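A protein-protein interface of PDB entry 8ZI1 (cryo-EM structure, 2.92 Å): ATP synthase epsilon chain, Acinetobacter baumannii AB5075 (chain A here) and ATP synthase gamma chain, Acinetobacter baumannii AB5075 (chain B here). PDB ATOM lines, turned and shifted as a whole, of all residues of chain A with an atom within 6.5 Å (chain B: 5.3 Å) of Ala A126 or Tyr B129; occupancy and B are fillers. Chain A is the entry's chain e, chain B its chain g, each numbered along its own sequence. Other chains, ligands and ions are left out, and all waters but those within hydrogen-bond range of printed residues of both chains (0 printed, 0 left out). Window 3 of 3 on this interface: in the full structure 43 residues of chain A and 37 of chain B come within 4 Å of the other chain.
Of chain B, only Tyr B129 (3.4 Å) comes within 4 Å of Ala A126. Of chain A, only Asp A113, Leu A118, Glu A123 and Ala A126 come within 4 Å of Tyr B129. Of the printed residues of chain B, Asp A113 touches Tyr B129 (3.9 Å), Gly B130 (3.4 Å) and Gly B131 (2.9 Å). Printed residues of chain B within 4 Å of Lys A109: Asn B128 (3.9 Å). Printed residues of chain A within 4 Å of Asn B128: Lys A109 and Asp A111. Of the printed residues of chain A, Gly B130 touches Asp A111 and Asp A113. Of the printed residues of chain A, Gly B131 touches Asp A113. Ile A131 touches none of the printed residues of chain B. Glu A129 touches none of the printed residues of chain B. The nearest residue of chain B that does not touch Ala A126 is Phe B125 (4.3 Å). The nearest printed residue of chain B that does not touch Leu A118 is Gly B130 (4.03 Å).
Printed residues of chain A that touch a printed residue of chain B: Lys A109, Asp A111, Asp A113, Leu A118, Glu A123 and Ala A126. Hydrophobic or aromatic side chains of chain A that line the printed part of chain B: Leu A118 and Ala A126. Along chain A the printed residues that touch a printed residue of chain B span positions 109 to 126. Among the printed residues, no Asp or Glu carboxylate lies within 4 Å of a Lys or Arg side-chain nitrogen of the other chain.
The backbone carbonyl oxygen (O) of Lys B127 sits close to the side-chain carboxylate (OD2) of Asp A111. The backbone carbonyl oxygen (O) of Asp A113 is in hydrogen-bond range of the backbone NH (N) of Gly B131 (2.9 Å).
The backbone carbonyl oxygen (O) of Phe B125 lies within hydrogen-bond range of the side-chain amide nitrogen (ND2) of Asn B128 (2.5 Å). O of Ala A126 lies within hydrogen-bond range of OG1 of Thr A130 (2.7 Å).
Among the printed residues, pairs that only touch across the chains: Glu A123 with Tyr B129 (3.2 Å), Leu A118 with Tyr B129 (3.3 Å), Asp A111 with Gly B130 (3.4 Å), Ala A126 with Tyr B129 (3.4 Å), Asp A113 with Gly B130 (3.4 Å), Lys A109 with Asn B128 (3.9 Å), Asp A113 with Tyr B129 (3.9 Å) and Asp A111 with Asn B128 (3.98 Å).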
ATOM      1  N   LYS A 109     -14.680  -0.476 -38.083  1.00  0.00           N
ATOM      2  CA  LYS A 109     -14.616  -1.757 -37.326  1.00  0.00           C
ATOM      3  C   LYS A 109     -15.010  -2.913 -38.252  1.00  0.00           C
ATOM      4  O   LYS A 109     -16.148  -2.903 -38.754  1.00  0.00           O
ATOM      5  CB  LYS A 109     -15.567  -1.710 -36.125  1.00  0.00           C
ATOM      6  CG  LYS A 109     -15.277  -0.627 -35.097  1.00  0.00           C
ATOM      7  CD  LYS A 109     -13.944  -0.799 -34.402  1.00  0.00           C
ATOM      8  CE  LYS A 109     -13.696   0.241 -33.331  1.00  0.00           C
ATOM      9  NZ  LYS A 109     -12.375   0.061 -32.686  1.00  0.00           N
ATOM     10  N   ASP A 111     -15.014  -6.169 -37.303  1.00  0.00           N
ATOM     11  CA  ASP A 111     -15.287  -7.363 -36.458  1.00  0.00           C
ATOM     12  C   ASP A 111     -16.508  -8.107 -37.009  1.00  0.00           C
ATOM     13  O   ASP A 111     -16.473  -9.352 -37.015  1.00  0.00           O
ATOM     14  CB  ASP A 111     -15.468  -6.966 -34.991  1.00  0.00           C
ATOM     15  CG  ASP A 111     -16.318  -5.721 -34.786  1.00  0.00           C
ATOM     16  OD1 ASP A 111     -16.963  -5.276 -35.757  1.00  0.00           O
ATOM     17  OD2 ASP A 111     -16.332  -5.209 -33.650  1.00  0.00           O
ATOM     18  N   ASP A 113     -18.948  -9.216 -35.935  1.00  0.00           N
ATOM     19  CA  ASP A 113     -19.334 -10.315 -35.060  1.00  0.00           C
ATOM     20  C   ASP A 113     -20.651  -9.979 -34.378  1.00  0.00           C
ATOM     21  O   ASP A 113     -20.838  -8.855 -33.899  1.00  0.00           O
ATOM     22  CB  ASP A 113     -18.250 -10.596 -34.015  1.00  0.00           C
ATOM     23  CG  ASP A 113     -17.692  -9.329 -33.396  1.00  0.00           C
ATOM     24  OD1 ASP A 113     -18.083  -8.228 -33.836  1.00  0.00           O
ATOM     25  OD2 ASP A 113     -16.862  -9.433 -32.469  1.00  0.00           O
ATOM     26  N   LEU A 118     -22.149 -10.172 -25.802  1.00  0.00           N
ATOM     27  CA  LEU A 118     -20.850 -10.811 -25.634  1.00  0.00           C
ATOM     28  C   LEU A 118     -20.000 -10.053 -24.624  1.00  0.00           C
ATOM     29  O   LEU A 118     -20.064  -8.822 -24.533  1.00  0.00           O
ATOM     30  CB  LEU A 118     -20.110 -10.895 -26.970  1.00  0.00           C
ATOM     31  CG  LEU A 118     -19.429  -9.638 -27.526  1.00  0.00           C
ATOM     32  CD1 LEU A 118     -18.450 -10.012 -28.630  1.00  0.00           C
ATOM     33  CD2 LEU A 118     -20.428  -8.604 -28.020  1.00  0.00           C
ATOM     34  N   ALA A 119     -19.205 -10.804 -23.861  1.00  0.00           N
ATOM     35  CA  ALA A 119     -18.209 -10.241 -22.950  1.00  0.00           C
ATOM     36  C   ALA A 119     -18.825  -9.214 -22.004  1.00  0.00           C
ATOM     37  O   ALA A 119     -18.252  -8.154 -21.750  1.00  0.00           O
ATOM     38  CB  ALA A 119     -17.042  -9.631 -23.727  1.00  0.00           C
ATOM     39  N   LEU A 121     -18.983  -9.407 -18.916  1.00  0.00           N
ATOM     40  CA  LEU A 121     -18.009  -9.212 -17.847  1.00  0.00           C
ATOM     41  C   LEU A 121     -16.979  -8.159 -18.235  1.00  0.00           C
ATOM     42  O   LEU A 121     -16.578  -7.334 -17.406  1.00  0.00           O
ATOM     43  CB  LEU A 121     -17.323 -10.537 -17.511  1.00  0.00           C
ATOM     44  CG  LEU A 121     -18.084 -11.544 -16.642  1.00  0.00           C
ATOM     45  CD1 LEU A 121     -19.172 -12.257 -17.434  1.00  0.00           C
ATOM     46  CD2 LEU A 121     -17.122 -12.551 -16.026  1.00  0.00           C
ATOM     47  N   ALA A 122     -16.536  -8.173 -19.496  1.00  0.00           N
ATOM     48  CA  ALA A 122     -15.600  -7.156 -19.962  1.00  0.00           C
ATOM     49  C   ALA A 122     -16.235  -5.770 -19.944  1.00  0.00           C
ATOM     50  O   ALA A 122     -15.575  -4.785 -19.592  1.00  0.00           O
ATOM     51  CB  ALA A 122     -15.100  -7.503 -21.364  1.00  0.00           C
ATOM     52  N   GLU A 123     -17.511  -5.672 -20.324  1.00  0.00           N
ATOM     53  CA  GLU A 123     -18.198  -4.385 -20.258  1.00  0.00           C
ATOM     54  C   GLU A 123     -18.307  -3.893 -18.822  1.00  0.00           C
ATOM     55  O   GLU A 123     -18.118  -2.702 -18.549  1.00  0.00           O
ATOM     56  CB  GLU A 123     -19.584  -4.487 -20.897  1.00  0.00           C
ATOM     57  CG  GLU A 123     -19.649  -5.399 -22.109  1.00  0.00           C
ATOM     58  CD  GLU A 123     -19.095  -4.754 -23.365  1.00  0.00           C
ATOM     59  OE1 GLU A 123     -18.701  -3.571 -23.311  1.00  0.00           O
ATOM     60  OE2 GLU A 123     -19.053  -5.436 -24.410  1.00  0.00           O
ATOM     61  N   THR A 124     -18.612  -4.796 -17.887  1.00  0.00           N
ATOM     62  CA  THR A 124     -18.679  -4.405 -16.482  1.00  0.00           C
ATOM     63  C   THR A 124     -17.314  -3.960 -15.969  1.00  0.00           C
ATOM     64  O   THR A 124     -17.214  -2.991 -15.206  1.00  0.00           O
ATOM     65  CB  THR A 124     -19.222  -5.561 -15.641  1.00  0.00           C
ATOM     66  OG1 THR A 124     -20.512  -5.944 -16.134  1.00  0.00           O
ATOM     67  CG2 THR A 124     -19.349  -5.147 -14.182  1.00  0.00           C
ATOM     68  N   ALA A 125     -16.251  -4.654 -16.377  1.00  0.00           N
ATOM     69  CA  ALA A 125     -14.905  -4.255 -15.974  1.00  0.00           C
ATOM     70  C   ALA A 125     -14.545  -2.884 -16.535  1.00  0.00           C
ATOM     71  O   ALA A 125     -13.931  -2.063 -15.845  1.00  0.00           O
ATOM     72  CB  ALA A 125     -13.890  -5.305 -16.423  1.00  0.00           C
ATOM     73  N   ALA A 126     -14.915  -2.623 -17.791  1.00  0.00           N
ATOM     74  CA  ALA A 126     -14.693  -1.302 -18.368  1.00  0.00           C
ATOM     75  C   ALA A 126     -15.483  -0.238 -17.618  1.00  0.00           C
ATOM     76  O   ALA A 126     -14.996   0.879 -17.409  1.00  0.00           O
ATOM     77  CB  ALA A 126     -15.065  -1.306 -19.850  1.00  0.00           C
ATOM     78  N   GLN A 127     -16.710  -0.568 -17.208  1.00  0.00           N
ATOM     79  CA  GLN A 127     -17.501   0.345 -16.393  1.00  0.00           C
ATOM     80  C   GLN A 127     -16.784   0.669 -15.088  1.00  0.00           C
ATOM     81  O   GLN A 127     -16.688   1.836 -14.689  1.00  0.00           O
ATOM     82  CB  GLN A 127     -18.872  -0.268 -16.113  1.00  0.00           C
ATOM     83  CG  GLN A 127     -19.891   0.690 -15.520  1.00  0.00           C
ATOM     84  CD  GLN A 127     -19.935   0.631 -14.006  1.00  0.00           C
ATOM     85  OE1 GLN A 127     -19.542  -0.365 -13.400  1.00  0.00           O
ATOM     86  NE2 GLN A 127     -20.425   1.698 -13.387  1.00  0.00           N
ATOM     87  N   LEU A 128     -16.263  -0.359 -14.417  1.00  0.00           N
ATOM     88  CA  LEU A 128     -15.550  -0.143 -13.162  1.00  0.00           C
ATOM     89  C   LEU A 128     -14.308   0.712 -13.372  1.00  0.00           C
ATOM     90  O   LEU A 128     -14.004   1.591 -12.556  1.00  0.00           O
ATOM     91  CB  LEU A 128     -15.173  -1.484 -12.531  1.00  0.00           C
ATOM     92  CG  LEU A 128     -16.324  -2.447 -12.236  1.00  0.00           C
ATOM     93  CD1 LEU A 128     -15.806  -3.734 -11.612  1.00  0.00           C
ATOM     94  CD2 LEU A 128     -17.355  -1.784 -11.337  1.00  0.00           C
ATOM     95  N   GLU A 129     -13.574   0.467 -14.460  1.00  0.00           N
ATOM     96  CA  GLU A 129     -12.390   1.270 -14.749  1.00  0.00           C
ATOM     97  C   GLU A 129     -12.761   2.722 -15.027  1.00  0.00           C
ATOM     98  O   GLU A 129     -12.049   3.642 -14.605  1.00  0.00           O
ATOM     99  CB  GLU A 129     -11.624   0.676 -15.930  1.00  0.00           C
ATOM    100  CG  GLU A 129     -11.032  -0.696 -15.656  1.00  0.00           C
ATOM    101  CD  GLU A 129      -9.951  -0.663 -14.595  1.00  0.00           C
ATOM    102  OE1 GLU A 129      -9.229   0.354 -14.510  1.00  0.00           O
ATOM    103  OE2 GLU A 129      -9.823  -1.652 -13.844  1.00  0.00           O
ATOM    104  N   THR A 130     -13.867   2.948 -15.736  1.00  0.00           N
ATOM    105  CA  THR A 130     -14.283   4.312 -16.043  1.00  0.00           C
ATOM    106  C   THR A 130     -14.833   5.025 -14.814  1.00  0.00           C
ATOM    107  O   THR A 130     -14.807   6.260 -14.756  1.00  0.00           O
ATOM    108  CB  THR A 130     -15.323   4.308 -17.161  1.00  0.00           C
ATOM    109  OG1 THR A 130     -16.275   3.263 -16.926  1.00  0.00           O
ATOM    110  CG2 THR A 130     -14.654   4.076 -18.508  1.00  0.00           C
ATOM    111  N   ILE A 131     -15.339   4.273 -13.833  1.00  0.00           N
ATOM    112  CA  ILE A 131     -15.824   4.892 -12.601  1.00  0.00           C
ATOM    113  C   ILE A 131     -14.685   5.590 -11.869  1.00  0.00           C
ATOM    114  O   ILE A 131     -14.866   6.671 -11.293  1.00  0.00           O
ATOM    115  CB  ILE A 131     -16.520   3.846 -11.711  1.00  0.00           C
ATOM    116  CG1 ILE A 131     -17.860   3.435 -12.320  1.00  0.00           C
ATOM    117  CG2 ILE A 131     -16.727   4.379 -10.301  1.00  0.00           C
ATOM    118  CD1 ILE A 131     -18.831   4.583 -12.481  1.00  0.00           C
ATOM    119  N   PHE B 125     -16.227   3.567 -29.216  1.00  0.00           N
ATOM    120  CA  PHE B 125     -15.957   2.776 -28.023  1.00  0.00           C
ATOM    121  C   PHE B 125     -16.797   1.511 -27.939  1.00  0.00           C
ATOM    122  O   PHE B 125     -16.251   0.420 -27.760  1.00  0.00           O
ATOM    123  CB  PHE B 125     -16.184   3.630 -26.765  1.00  0.00           C
ATOM    124  CG  PHE B 125     -16.116   2.851 -25.479  1.00  0.00           C
ATOM    125  CD1 PHE B 125     -14.895   2.566 -24.892  1.00  0.00           C
ATOM    126  CD2 PHE B 125     -17.272   2.413 -24.852  1.00  0.00           C
ATOM    127  CE1 PHE B 125     -14.827   1.854 -23.709  1.00  0.00           C
ATOM    128  CE2 PHE B 125     -17.212   1.699 -23.671  1.00  0.00           C
ATOM    129  CZ  PHE B 125     -15.987   1.421 -23.098  1.00  0.00           C
ATOM    130  N   PHE B 126     -18.119   1.630 -28.060  1.00  0.00           N
ATOM    131  CA  PHE B 126     -18.991   0.482 -27.840  1.00  0.00           C
ATOM    132  C   PHE B 126     -18.826  -0.589 -28.913  1.00  0.00           C
ATOM    133  O   PHE B 126     -19.223  -1.736 -28.689  1.00  0.00           O
ATOM    134  CB  PHE B 126     -20.446   0.948 -27.762  1.00  0.00           C
ATOM    135  CG  PHE B 126     -21.430  -0.162 -27.547  1.00  0.00           C
ATOM    136  CD1 PHE B 126     -21.436  -0.877 -26.363  1.00  0.00           C
ATOM    137  CD2 PHE B 126     -22.351  -0.486 -28.526  1.00  0.00           C
ATOM    138  CE1 PHE B 126     -22.341  -1.898 -26.159  1.00  0.00           C
ATOM    139  CE2 PHE B 126     -23.259  -1.506 -28.330  1.00  0.00           C
ATOM    140  CZ  PHE B 126     -23.253  -2.212 -27.144  1.00  0.00           C
ATOM    141  N   LYS B 127     -18.275  -0.214 -30.069  1.00  0.00           N
ATOM    142  CA  LYS B 127     -18.206  -1.189 -31.191  1.00  0.00           C
ATOM    143  C   LYS B 127     -16.898  -1.984 -31.150  1.00  0.00           C
ATOM    144  O   LYS B 127     -16.843  -3.034 -31.809  1.00  0.00           O
ATOM    145  CB  LYS B 127     -18.398  -0.479 -32.533  1.00  0.00           C
ATOM    146  CG  LYS B 127     -19.740   0.223 -32.683  1.00  0.00           C
ATOM    147  CD  LYS B 127     -20.912  -0.737 -32.662  1.00  0.00           C
ATOM    148  CE  LYS B 127     -22.248  -0.059 -32.882  1.00  0.00           C
ATOM    149  NZ  LYS B 127     -23.367  -1.028 -32.831  1.00  0.00           N
ATOM    150  N   ASN B 128     -15.897  -1.522 -30.396  1.00  0.00           N
ATOM    151  CA  ASN B 128     -14.660  -2.335 -30.259  1.00  0.00           C
ATOM    152  C   ASN B 128     -15.073  -3.715 -29.741  1.00  0.00           C
ATOM    153  O   ASN B 128     -14.466  -4.714 -30.167  1.00  0.00           O
ATOM    154  CB  ASN B 128     -13.593  -1.645 -29.400  1.00  0.00           C
ATOM    155  CG  ASN B 128     -13.777  -1.801 -27.903  1.00  0.00           C
ATOM    156  OD1 ASN B 128     -13.618  -2.889 -27.353  1.00  0.00           O
ATOM    157  ND2 ASN B 128     -14.067  -0.704 -27.225  1.00  0.00           N
ATOM    158  N   TYR B 129     -16.082  -3.758 -28.869  1.00  0.00           N
ATOM    159  CA  TYR B 129     -16.547  -5.040 -28.284  1.00  0.00           C
ATOM    160  C   TYR B 129     -17.252  -5.872 -29.357  1.00  0.00           C
ATOM    161  O   TYR B 129     -17.092  -7.103 -29.347  1.00  0.00           O
ATOM    162  CB  TYR B 129     -17.442  -4.744 -27.082  1.00  0.00           C
ATOM    163  CG  TYR B 129     -16.755  -3.896 -26.044  1.00  0.00           C
ATOM    164  CD1 TYR B 129     -15.828  -4.451 -25.182  1.00  0.00           C
ATOM    165  CD2 TYR B 129     -17.001  -2.536 -25.947  1.00  0.00           C
ATOM    166  CE1 TYR B 129     -15.176  -3.686 -24.231  1.00  0.00           C
ATOM    167  CE2 TYR B 129     -16.358  -1.755 -25.002  1.00  0.00           C
ATOM    168  CZ  TYR B 129     -15.442  -2.332 -24.142  1.00  0.00           C
ATOM    169  OH  TYR B 129     -14.796  -1.579 -23.206  1.00  0.00           O
ATOM    170  N   GLY B 130     -17.987  -5.221 -30.260  1.00  0.00           N
ATOM    171  CA  GLY B 130     -18.656  -5.951 -31.353  1.00  0.00           C
ATOM    172  C   GLY B 130     -20.164  -5.874 -31.240  1.00  0.00           C
ATOM    173  O   GLY B 130     -20.693  -5.285 -30.282  1.00  0.00           O
ATOM    174  N   GLY B 131     -20.891  -6.483 -32.181  1.00  0.00           N
ATOM    175  CA  GLY B 131     -22.360  -6.345 -32.177  1.00  0.00           C
ATOM    176  C   GLY B 131     -22.923  -6.251 -33.583  1.00  0.00           C
ATOM    177  O   GLY B 131     -22.320  -5.536 -34.408  1.00  0.00           O
